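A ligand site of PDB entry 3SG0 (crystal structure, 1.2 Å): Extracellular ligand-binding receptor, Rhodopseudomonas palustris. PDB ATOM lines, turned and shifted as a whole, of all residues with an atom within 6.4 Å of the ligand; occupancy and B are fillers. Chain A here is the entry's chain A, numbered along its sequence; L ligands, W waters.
N of Ala 121 sits at hydrogen-bond distance from O1 of the ligand (3.0 Å).
O2 of the ligand lies within salt-bridge range of NH2 of Arg 198 (2.8 Å).
An oxygen (O2) of the ligand sits at hydrogen-bond distance from the backbone NH of Thr 99 (2.7 Å).
An oxygen (O1) of the ligand lies within hydrogen-bond range of the side-chain hydroxyl of Thr 99, at 2.7 Å.
The backbone carbonyl oxygen (O) of Leu 43 sits close to the side-chain amide nitrogen (NE2) of Gln 47, at 3.4 Å.
OH of Tyr 171 sits at hydrogen-bond distance from OG1 of Thr 246 (2.7 Å).
The backbone NH (N) of Gly 248 lies close to the side-chain hydroxyl (OG1) of Thr 246, 3.2 Å away.
The backbone NH of Tyr 171 lies within hydrogen-bond range of the side-chain carboxylate of Asp 169 (2.9 Å).
The side-chain sulfur (SD) of Met 119 lies close to the side-chain amide oxygen (OE1) of Gln 47 (3.8 Å).
The side-chain hydroxyl (OG) of Ser 97 lies within hydrogen-bond range of the side-chain amide oxygen (OE1) of Gln 47.
The backbone NH (N) of Ala 122 sits at hydrogen-bond distance from the side-chain hydroxyl (OG1) of Thr 99, at 3.2 Å.
The guanidinium group of Arg 198 is in salt-bridge range of the side-chain carboxylate of Asp 169 (3.0 Å).
Residues that only touch the ligand: Ala 223 (3.0 Å), Ser 97 (3.3 Å), Leu 98 (3.4 Å), Tyr 171 (3.4 Å), Ala 120 (3.5 Å), Met 119 (3.5 Å), His 247 (3.6 Å), Gly 248 (3.6 Å), Leu 43 (3.6 Å), Phe 307 (3.7 Å), Pro 100 (3.9 Å), Val 140 (3.9 Å) and His 310 (3.97 Å).
Hydrophobic or aromatic side chains within 4 Å of the ligand: Leu 43, Leu 98, Pro 100, Ala 120, Ala 121, Val 140, Tyr 171, Ala 223, His 247, Phe 307 and His 310.
Water W1 lies within hydrogen-bond range of OE1 of Glu 270 (2.9 Å) and O of His 247 (3.3 Å).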
ATOM      1  N   LEU A  43      25.584 -20.061   7.918  1.00  0.00           N
ATOM      2  CA  LEU A  43      24.575 -19.778   8.935  1.00  0.00           C
ATOM      3  C   LEU A  43      25.066 -18.683   9.890  1.00  0.00           C
ATOM      4  O   LEU A  43      24.353 -17.713  10.173  1.00  0.00           O
ATOM      5  CB  LEU A  43      24.161 -21.038   9.709  1.00  0.00           C
ATOM      6  CG  LEU A  43      23.512 -22.163   8.897  1.00  0.00           C
ATOM      7  CD1 LEU A  43      24.544 -23.029   8.160  1.00  0.00           C
ATOM      8  CD2 LEU A  43      22.634 -23.035   9.780  1.00  0.00           C
ATOM      9  N   GLN A  47      24.397 -14.156  10.821  1.00  0.00           N
ATOM     10  CA  GLN A  47      24.094 -13.802  12.204  1.00  0.00           C
ATOM     11  C   GLN A  47      25.076 -12.745  12.714  1.00  0.00           C
ATOM     12  O   GLN A  47      24.673 -11.759  13.315  1.00  0.00           O
ATOM     13  CB  GLN A  47      24.056 -15.058  13.065  1.00  0.00           C
ATOM     14  CG  GLN A  47      22.871 -15.943  12.661  1.00  0.00           C
ATOM     15  CD  GLN A  47      23.005 -17.391  13.015  1.00  0.00           C
ATOM     16  OE1 GLN A  47      23.979 -17.828  13.640  1.00  0.00           O
ATOM     17  NE2 GLN A  47      22.015 -18.174  12.606  1.00  0.00           N
ATOM     18  N   SER A  97      24.679 -21.595  16.129  1.00  0.00           N
ATOM     19  CA  SER A  97      24.048 -21.686  14.820  1.00  0.00           C
ATOM     20  C   SER A  97      23.653 -23.104  14.435  1.00  0.00           C
ATOM     21  O   SER A  97      22.781 -23.294  13.585  1.00  0.00           O
ATOM     22  CB  SER A  97      25.017 -21.199  13.749  1.00  0.00           C
ATOM     23  OG  SER A  97      25.566 -19.935  14.059  1.00  0.00           O
ATOM     24  N   LEU A  98      24.347 -24.078  15.016  1.00  0.00           N
ATOM     25  CA  LEU A  98      24.220 -25.483  14.617  1.00  0.00           C
ATOM     26  C   LEU A  98      23.818 -26.321  15.817  1.00  0.00           C
ATOM     27  O   LEU A  98      24.114 -25.975  16.956  1.00  0.00           O
ATOM     28  CB  LEU A  98      25.548 -26.036  14.087  1.00  0.00           C
ATOM     29  CG  LEU A  98      26.363 -25.157  13.137  1.00  0.00           C
ATOM     30  CD1 LEU A  98      27.633 -25.901  12.691  1.00  0.00           C
ATOM     31  CD2 LEU A  98      25.531 -24.730  11.950  1.00  0.00           C
ATOM     32  N   THR A  99      23.175 -27.441  15.539  1.00  0.00           N
ATOM     33  CA  THR A  99      22.693 -28.326  16.587  1.00  0.00           C
ATOM     34  C   THR A  99      23.812 -28.928  17.449  1.00  0.00           C
ATOM     35  O   THR A  99      23.750 -28.835  18.679  1.00  0.00           O
ATOM     36  CB  THR A  99      21.754 -29.402  16.008  1.00  0.00           C
ATOM     37  OG1 THR A  99      20.555 -28.772  15.548  1.00  0.00           O
ATOM     38  CG2 THR A  99      21.395 -30.419  17.068  1.00  0.00           C
ATOM     39  N   PRO A 100      24.830 -29.562  16.842  1.00  0.00           N
ATOM     40  CA  PRO A 100      25.885 -30.147  17.681  1.00  0.00           C
ATOM     41  C   PRO A 100      26.582 -29.101  18.550  1.00  0.00           C
ATOM     42  O   PRO A 100      27.021 -29.389  19.665  1.00  0.00           O
ATOM     43  CB  PRO A 100      26.872 -30.748  16.665  1.00  0.00           C
ATOM     44  CG  PRO A 100      26.552 -30.072  15.353  1.00  0.00           C
ATOM     45  CD  PRO A 100      25.077 -29.799  15.407  1.00  0.00           C
ATOM     46  N   MET A 119      19.831 -20.776  18.074  1.00  0.00           N
ATOM     47  CA  MET A 119      19.540 -20.448  16.674  1.00  0.00           C
ATOM     48  C   MET A 119      19.539 -21.681  15.765  1.00  0.00           C
ATOM     49  O   MET A 119      19.402 -21.553  14.546  1.00  0.00           O
ATOM     50  CB  MET A 119      20.497 -19.375  16.157  1.00  0.00           C
ATOM     51  CG  MET A 119      20.388 -18.062  16.920  1.00  0.00           C
ATOM     52  SD  MET A 119      21.517 -16.650  16.243  1.00  0.00           S
ATOM     53  CE  MET A 119      23.241 -17.343  16.850  1.00  0.00           C
ATOM     54  N   ALA A 120      19.661 -22.863  16.366  1.00  0.00           N
ATOM     55  CA  ALA A 120      19.742 -24.102  15.616  1.00  0.00           C
ATOM     56  C   ALA A 120      18.373 -24.787  15.518  1.00  0.00           C
ATOM     57  O   ALA A 120      17.385 -24.269  16.062  1.00  0.00           O
ATOM     58  CB  ALA A 120      20.780 -25.013  16.245  1.00  0.00           C
ATOM     59  N   ALA A 121      18.320 -25.922  14.842  1.00  0.00           N
ATOM     60  CA  ALA A 121      17.034 -26.448  14.347  1.00  0.00           C
ATOM     61  C   ALA A 121      16.498 -27.719  14.988  1.00  0.00           C
ATOM     62  O   ALA A 121      15.280 -27.940  14.971  1.00  0.00           O
ATOM     63  CB  ALA A 121      17.121 -26.663  12.834  1.00  0.00           C
ATOM     64  N   ALA A 122      17.350 -28.602  15.497  1.00  0.00           N
ATOM     65  CA  ALA A 122      16.874 -29.930  15.914  1.00  0.00           C
ATOM     66  C   ALA A 122      15.909 -29.870  17.107  1.00  0.00           C
ATOM     67  O   ALA A 122      16.123 -29.132  18.050  1.00  0.00           O
ATOM     68  CB  ALA A 122      18.031 -30.837  16.230  1.00  0.00           C
ATOM     69  N   LEU A 125      16.826 -29.856  20.947  1.00  0.00           N
ATOM     70  CA  LEU A 125      17.307 -28.677  21.665  1.00  0.00           C
ATOM     71  C   LEU A 125      16.316 -28.170  22.718  1.00  0.00           C
ATOM     72  O   LEU A 125      16.743 -27.580  23.711  1.00  0.00           O
ATOM     73  CB  LEU A 125      17.680 -27.570  20.679  1.00  0.00           C
ATOM     74  CG  LEU A 125      18.860 -27.930  19.758  1.00  0.00           C
ATOM     75  CD1 LEU A 125      18.967 -26.938  18.613  1.00  0.00           C
ATOM     76  CD2 LEU A 125      20.156 -27.998  20.544  1.00  0.00           C
ATOM     77  N   VAL A 140      13.735 -21.239  15.434  1.00  0.00           N
ATOM     78  CA  VAL A 140      13.644 -22.033  14.202  1.00  0.00           C
ATOM     79  C   VAL A 140      12.671 -23.163  14.461  1.00  0.00           C
ATOM     80  O   VAL A 140      12.760 -23.828  15.481  1.00  0.00           O
ATOM     81  CB  VAL A 140      15.023 -22.615  13.809  1.00  0.00           C
ATOM     82  CG1 VAL A 140      14.876 -23.541  12.609  1.00  0.00           C
ATOM     83  CG2 VAL A 140      16.003 -21.492  13.501  1.00  0.00           C
ATOM     84  N   ASP A 143      12.695 -29.486  13.651  1.00  0.00           N
ATOM     85  CA  ASP A 143      12.864 -30.254  12.426  1.00  0.00           C
ATOM     86  C   ASP A 143      11.826 -31.345  12.259  1.00  0.00           C
ATOM     87  O   ASP A 143      11.534 -31.715  11.121  1.00  0.00           O
ATOM     88  CB  ASP A 143      14.257 -30.864  12.358  1.00  0.00           C
ATOM     89  CG  ASP A 143      15.318 -29.841  12.021  1.00  0.00           C
ATOM     90  OD1 ASP A 143      15.052 -28.985  11.135  1.00  0.00           O
ATOM     91  OD2 ASP A 143      16.394 -29.880  12.649  1.00  0.00           O
ATOM     92  N   PHE A 167      23.800 -35.498   7.439  1.00  0.00           N
ATOM     93  CA  PHE A 167      24.923 -35.322   8.338  1.00  0.00           C
ATOM     94  C   PHE A 167      24.895 -36.409   9.424  1.00  0.00           C
ATOM     95  O   PHE A 167      23.834 -36.779   9.931  1.00  0.00           O
ATOM     96  CB  PHE A 167      24.849 -33.985   9.059  1.00  0.00           C
ATOM     97  CG  PHE A 167      25.202 -32.778   8.205  1.00  0.00           C
ATOM     98  CD1 PHE A 167      26.069 -32.847   7.119  1.00  0.00           C
ATOM     99  CD2 PHE A 167      24.678 -31.549   8.559  1.00  0.00           C
ATOM    100  CE1 PHE A 167      26.386 -31.695   6.403  1.00  0.00           C
ATOM    101  CE2 PHE A 167      24.981 -30.407   7.854  1.00  0.00           C
ATOM    102  CZ  PHE A 167      25.851 -30.471   6.776  1.00  0.00           C
ATOM    103  N   ASP A 169      25.149 -36.312  12.520  1.00  0.00           N
ATOM    104  CA  ASP A 169      24.994 -35.605  13.780  1.00  0.00           C
ATOM    105  C   ASP A 169      23.519 -35.503  14.107  1.00  0.00           C
ATOM    106  O   ASP A 169      22.671 -36.034  13.379  1.00  0.00           O
ATOM    107  CB  ASP A 169      25.680 -34.227  13.750  1.00  0.00           C
ATOM    108  CG  ASP A 169      25.056 -33.255  12.742  1.00  0.00           C
ATOM    109  OD1 ASP A 169      23.868 -33.374  12.410  1.00  0.00           O
ATOM    110  OD2 ASP A 169      25.793 -32.345  12.305  1.00  0.00           O
ATOM    111  N   TYR A 171      21.395 -33.124  13.949  1.00  0.00           N
ATOM    112  CA  TYR A 171      20.562 -32.451  12.953  1.00  0.00           C
ATOM    113  C   TYR A 171      20.139 -33.432  11.860  1.00  0.00           C
ATOM    114  O   TYR A 171      18.945 -33.598  11.585  1.00  0.00           O
ATOM    115  CB  TYR A 171      21.297 -31.266  12.327  1.00  0.00           C
ATOM    116  CG  TYR A 171      20.505 -30.597  11.218  1.00  0.00           C
ATOM    117  CD1 TYR A 171      19.428 -29.777  11.514  1.00  0.00           C
ATOM    118  CD2 TYR A 171      20.814 -30.818   9.885  1.00  0.00           C
ATOM    119  CE1 TYR A 171      18.694 -29.178  10.515  1.00  0.00           C
ATOM    120  CE2 TYR A 171      20.090 -30.227   8.875  1.00  0.00           C
ATOM    121  CZ  TYR A 171      19.026 -29.404   9.189  1.00  0.00           C
ATOM    122  OH  TYR A 171      18.274 -28.785   8.222  1.00  0.00           O
ATOM    123  N   ARG A 198      30.221 -32.790   8.154  1.00  0.00           N
ATOM    124  CA  ARG A 198      29.987 -31.505   7.494  1.00  0.00           C
ATOM    125  C   ARG A 198      31.138 -31.019   6.614  1.00  0.00           C
ATOM    126  O   ARG A 198      30.904 -30.416   5.566  1.00  0.00           O
ATOM    127  CB  ARG A 198      29.581 -30.417   8.493  1.00  0.00           C
ATOM    128  CG  ARG A 198      28.366 -30.763   9.332  1.00  0.00           C
ATOM    129  CD  ARG A 198      27.667 -29.509   9.890  1.00  0.00           C
ATOM    130  NE  ARG A 198      26.553 -29.908  10.748  1.00  0.00           N
ATOM    131  CZ  ARG A 198      25.440 -29.214  10.965  1.00  0.00           C
ATOM    132  NH1 ARG A 198      25.237 -28.031  10.395  1.00  0.00           N
ATOM    133  NH2 ARG A 198      24.520 -29.727  11.758  1.00  0.00           N
ATOM    134  N   SER A 222      21.008 -31.801   5.330  1.00  0.00           N
ATOM    135  CA  SER A 222      22.252 -31.059   5.402  1.00  0.00           C
ATOM    136  C   SER A 222      21.956 -29.585   5.634  1.00  0.00           C
ATOM    137  O   SER A 222      20.798 -29.180   5.728  1.00  0.00           O
ATOM    138  CB  SER A 222      23.035 -31.291   4.116  1.00  0.00           C
ATOM    139  OG  SER A 222      24.299 -30.669   4.144  1.00  0.00           O
ATOM    140  N   ALA A 223      22.995 -28.768   5.726  1.00  0.00           N
ATOM    141  CA  ALA A 223      22.807 -27.341   5.971  1.00  0.00           C
ATOM    142  C   ALA A 223      24.024 -26.565   5.518  1.00  0.00           C
ATOM    143  O   ALA A 223      25.154 -27.074   5.564  1.00  0.00           O
ATOM    144  CB  ALA A 223      22.552 -27.074   7.440  1.00  0.00           C
ATOM    145  N   GLY A 224      23.795 -25.322   5.108  1.00  0.00           N
ATOM    146  CA  GLY A 224      24.878 -24.464   4.655  1.00  0.00           C
ATOM    147  C   GLY A 224      25.473 -24.928   3.341  1.00  0.00           C
ATOM    148  O   GLY A 224      24.892 -25.726   2.606  1.00  0.00           O
ATOM    149  N   THR A 246      16.456 -29.659   3.035  1.00  0.00           N
ATOM    150  CA  THR A 246      15.877 -29.143   4.272  1.00  0.00           C
ATOM    151  C   THR A 246      16.081 -27.639   4.337  1.00  0.00           C
ATOM    152  O   THR A 246      16.806 -27.064   3.531  1.00  0.00           O
ATOM    153  CB  THR A 246      16.549 -29.737   5.517  1.00  0.00           C
ATOM    154  OG1 THR A 246      17.896 -29.230   5.612  1.00  0.00           O
ATOM    155  CG2 THR A 246      16.548 -31.259   5.496  1.00  0.00           C
ATOM    156  N   HIS A 247      15.467 -27.007   5.337  1.00  0.00           N
ATOM    157  CA  HIS A 247      15.626 -25.574   5.516  1.00  0.00           C
ATOM    158  C   HIS A 247      17.049 -25.126   5.858  1.00  0.00           C
ATOM    159  O   HIS A 247      17.322 -23.938   5.925  1.00  0.00           O
ATOM    160  CB  HIS A 247      14.607 -25.008   6.518  1.00  0.00           C
ATOM    161  CG  HIS A 247      14.685 -25.603   7.898  1.00  0.00           C
ATOM    162  ND1 HIS A 247      13.872 -25.173   8.918  1.00  0.00           N
ATOM    163  CD2 HIS A 247      15.456 -26.590   8.418  1.00  0.00           C
ATOM    164  CE1 HIS A 247      14.135 -25.863  10.011  1.00  0.00           C
ATOM    165  NE2 HIS A 247      15.093 -26.734   9.744  1.00  0.00           N
ATOM    166  N   GLY A 248      17.959 -26.088   6.069  1.00  0.00           N
ATOM    167  CA  GLY A 248      19.377 -25.763   6.179  1.00  0.00           C
ATOM    168  C   GLY A 248      19.942 -25.185   4.895  1.00  0.00           C
ATOM    169  O   GLY A 248      21.034 -24.603   4.917  1.00  0.00           O
ATOM    170  N   VAL A 249      19.231 -25.320   3.770  1.00  0.00           N
ATOM    171  CA  VAL A 249      19.755 -24.835   2.500  1.00  0.00           C
ATOM    172  C   VAL A 249      19.171 -23.501   2.071  1.00  0.00           C
ATOM    173  O   VAL A 249      19.480 -23.008   0.980  1.00  0.00           O
ATOM    174  CB  VAL A 249      19.584 -25.869   1.354  1.00  0.00           C
ATOM    175  CG1 VAL A 249      20.059 -27.248   1.793  1.00  0.00           C
ATOM    176  CG2 VAL A 249      18.138 -25.904   0.831  1.00  0.00           C
ATOM    177  N   GLU A 270      10.537 -22.096   6.181  1.00  0.00           N
ATOM    178  CA  GLU A 270       9.913 -21.005   6.914  1.00  0.00           C
ATOM    179  C   GLU A 270       9.207 -19.993   6.038  1.00  0.00           C
ATOM    180  O   GLU A 270       9.552 -19.825   4.868  1.00  0.00           O
ATOM    181  CB  GLU A 270      10.975 -20.267   7.750  1.00  0.00           C
ATOM    182  CG  GLU A 270      11.499 -21.033   8.940  1.00  0.00           C
ATOM    183  CD  GLU A 270      12.444 -22.169   8.573  1.00  0.00           C
ATOM    184  OE1 GLU A 270      13.460 -21.922   7.875  1.00  0.00           O
ATOM    185  OE2 GLU A 270      12.156 -23.296   9.011  1.00  0.00           O
ATOM    186  N   PHE A 307      19.470 -16.920   7.624  1.00  0.00           N
ATOM    187  CA  PHE A 307      20.087 -17.294   8.888  1.00  0.00           C
ATOM    188  C   PHE A 307      20.250 -16.119   9.846  1.00  0.00           C
ATOM    189  O   PHE A 307      20.195 -16.307  11.054  1.00  0.00           O
ATOM    190  CB  PHE A 307      21.354 -18.124   8.661  1.00  0.00           C
ATOM    191  CG  PHE A 307      21.031 -19.407   7.986  1.00  0.00           C
ATOM    192  CD1 PHE A 307      21.243 -19.588   6.628  1.00  0.00           C
ATOM    193  CD2 PHE A 307      20.395 -20.417   8.699  1.00  0.00           C
ATOM    194  CE1 PHE A 307      20.848 -20.772   6.005  1.00  0.00           C
ATOM    195  CE2 PHE A 307      20.003 -21.583   8.077  1.00  0.00           C
ATOM    196  CZ  PHE A 307      20.224 -21.766   6.728  1.00  0.00           C
ATOM    197  N   HIS A 310      17.325 -15.661  12.282  1.00  0.00           N
ATOM    198  CA  HIS A 310      17.233 -16.481  13.485  1.00  0.00           C
ATOM    199  C   HIS A 310      17.744 -15.699  14.685  1.00  0.00           C
ATOM    200  O   HIS A 310      17.249 -15.869  15.804  1.00  0.00           O
ATOM    201  CB  HIS A 310      17.936 -17.814  13.265  1.00  0.00           C
ATOM    202  CG  HIS A 310      17.310 -18.560  12.138  1.00  0.00           C
ATOM    203  ND1 HIS A 310      17.937 -19.486  11.322  1.00  0.00           N
ATOM    204  CD2 HIS A 310      16.047 -18.447  11.673  1.00  0.00           C
ATOM    205  CE1 HIS A 310      17.077 -19.893  10.407  1.00  0.00           C
ATOM    206  NE2 HIS A 310      15.923 -19.286  10.608  1.00  0.00           N
HETATM  207  O1  LIG L   1      20.668 -27.086  13.465  1.00  0.00           O
HETATM  208  C1  LIG L   1      21.568 -27.226  12.687  1.00  0.00           C
HETATM  209  O2  LIG L   1      22.680 -28.024  12.939  1.00  0.00           O
HETATM  210  C2  LIG L   1      21.449 -26.723  11.269  1.00  0.00           C
HETATM  211  O3  LIG L   1      22.212 -27.085  10.425  1.00  0.00           O
HETATM  212  C3  LIG L   1      20.372 -25.714  10.993  1.00  0.00           C
HETATM  213  C4  LIG L   1      20.185 -24.550  11.958  1.00  0.00           C
HETATM  214  C5  LIG L   1      19.087 -23.538  11.714  1.00  0.00           C
HETATM  215  C6  LIG L   1      18.174 -23.707  10.503  1.00  0.00           C
HETATM  216  C7  LIG L   1      18.382 -24.904   9.550  1.00  0.00           C
HETATM  217  C8  LIG L   1      19.490 -25.911   9.776  1.00  0.00           C
HETATM  218  O   HOH W   1      16.386 -21.829   8.230  1.00  0.00           O
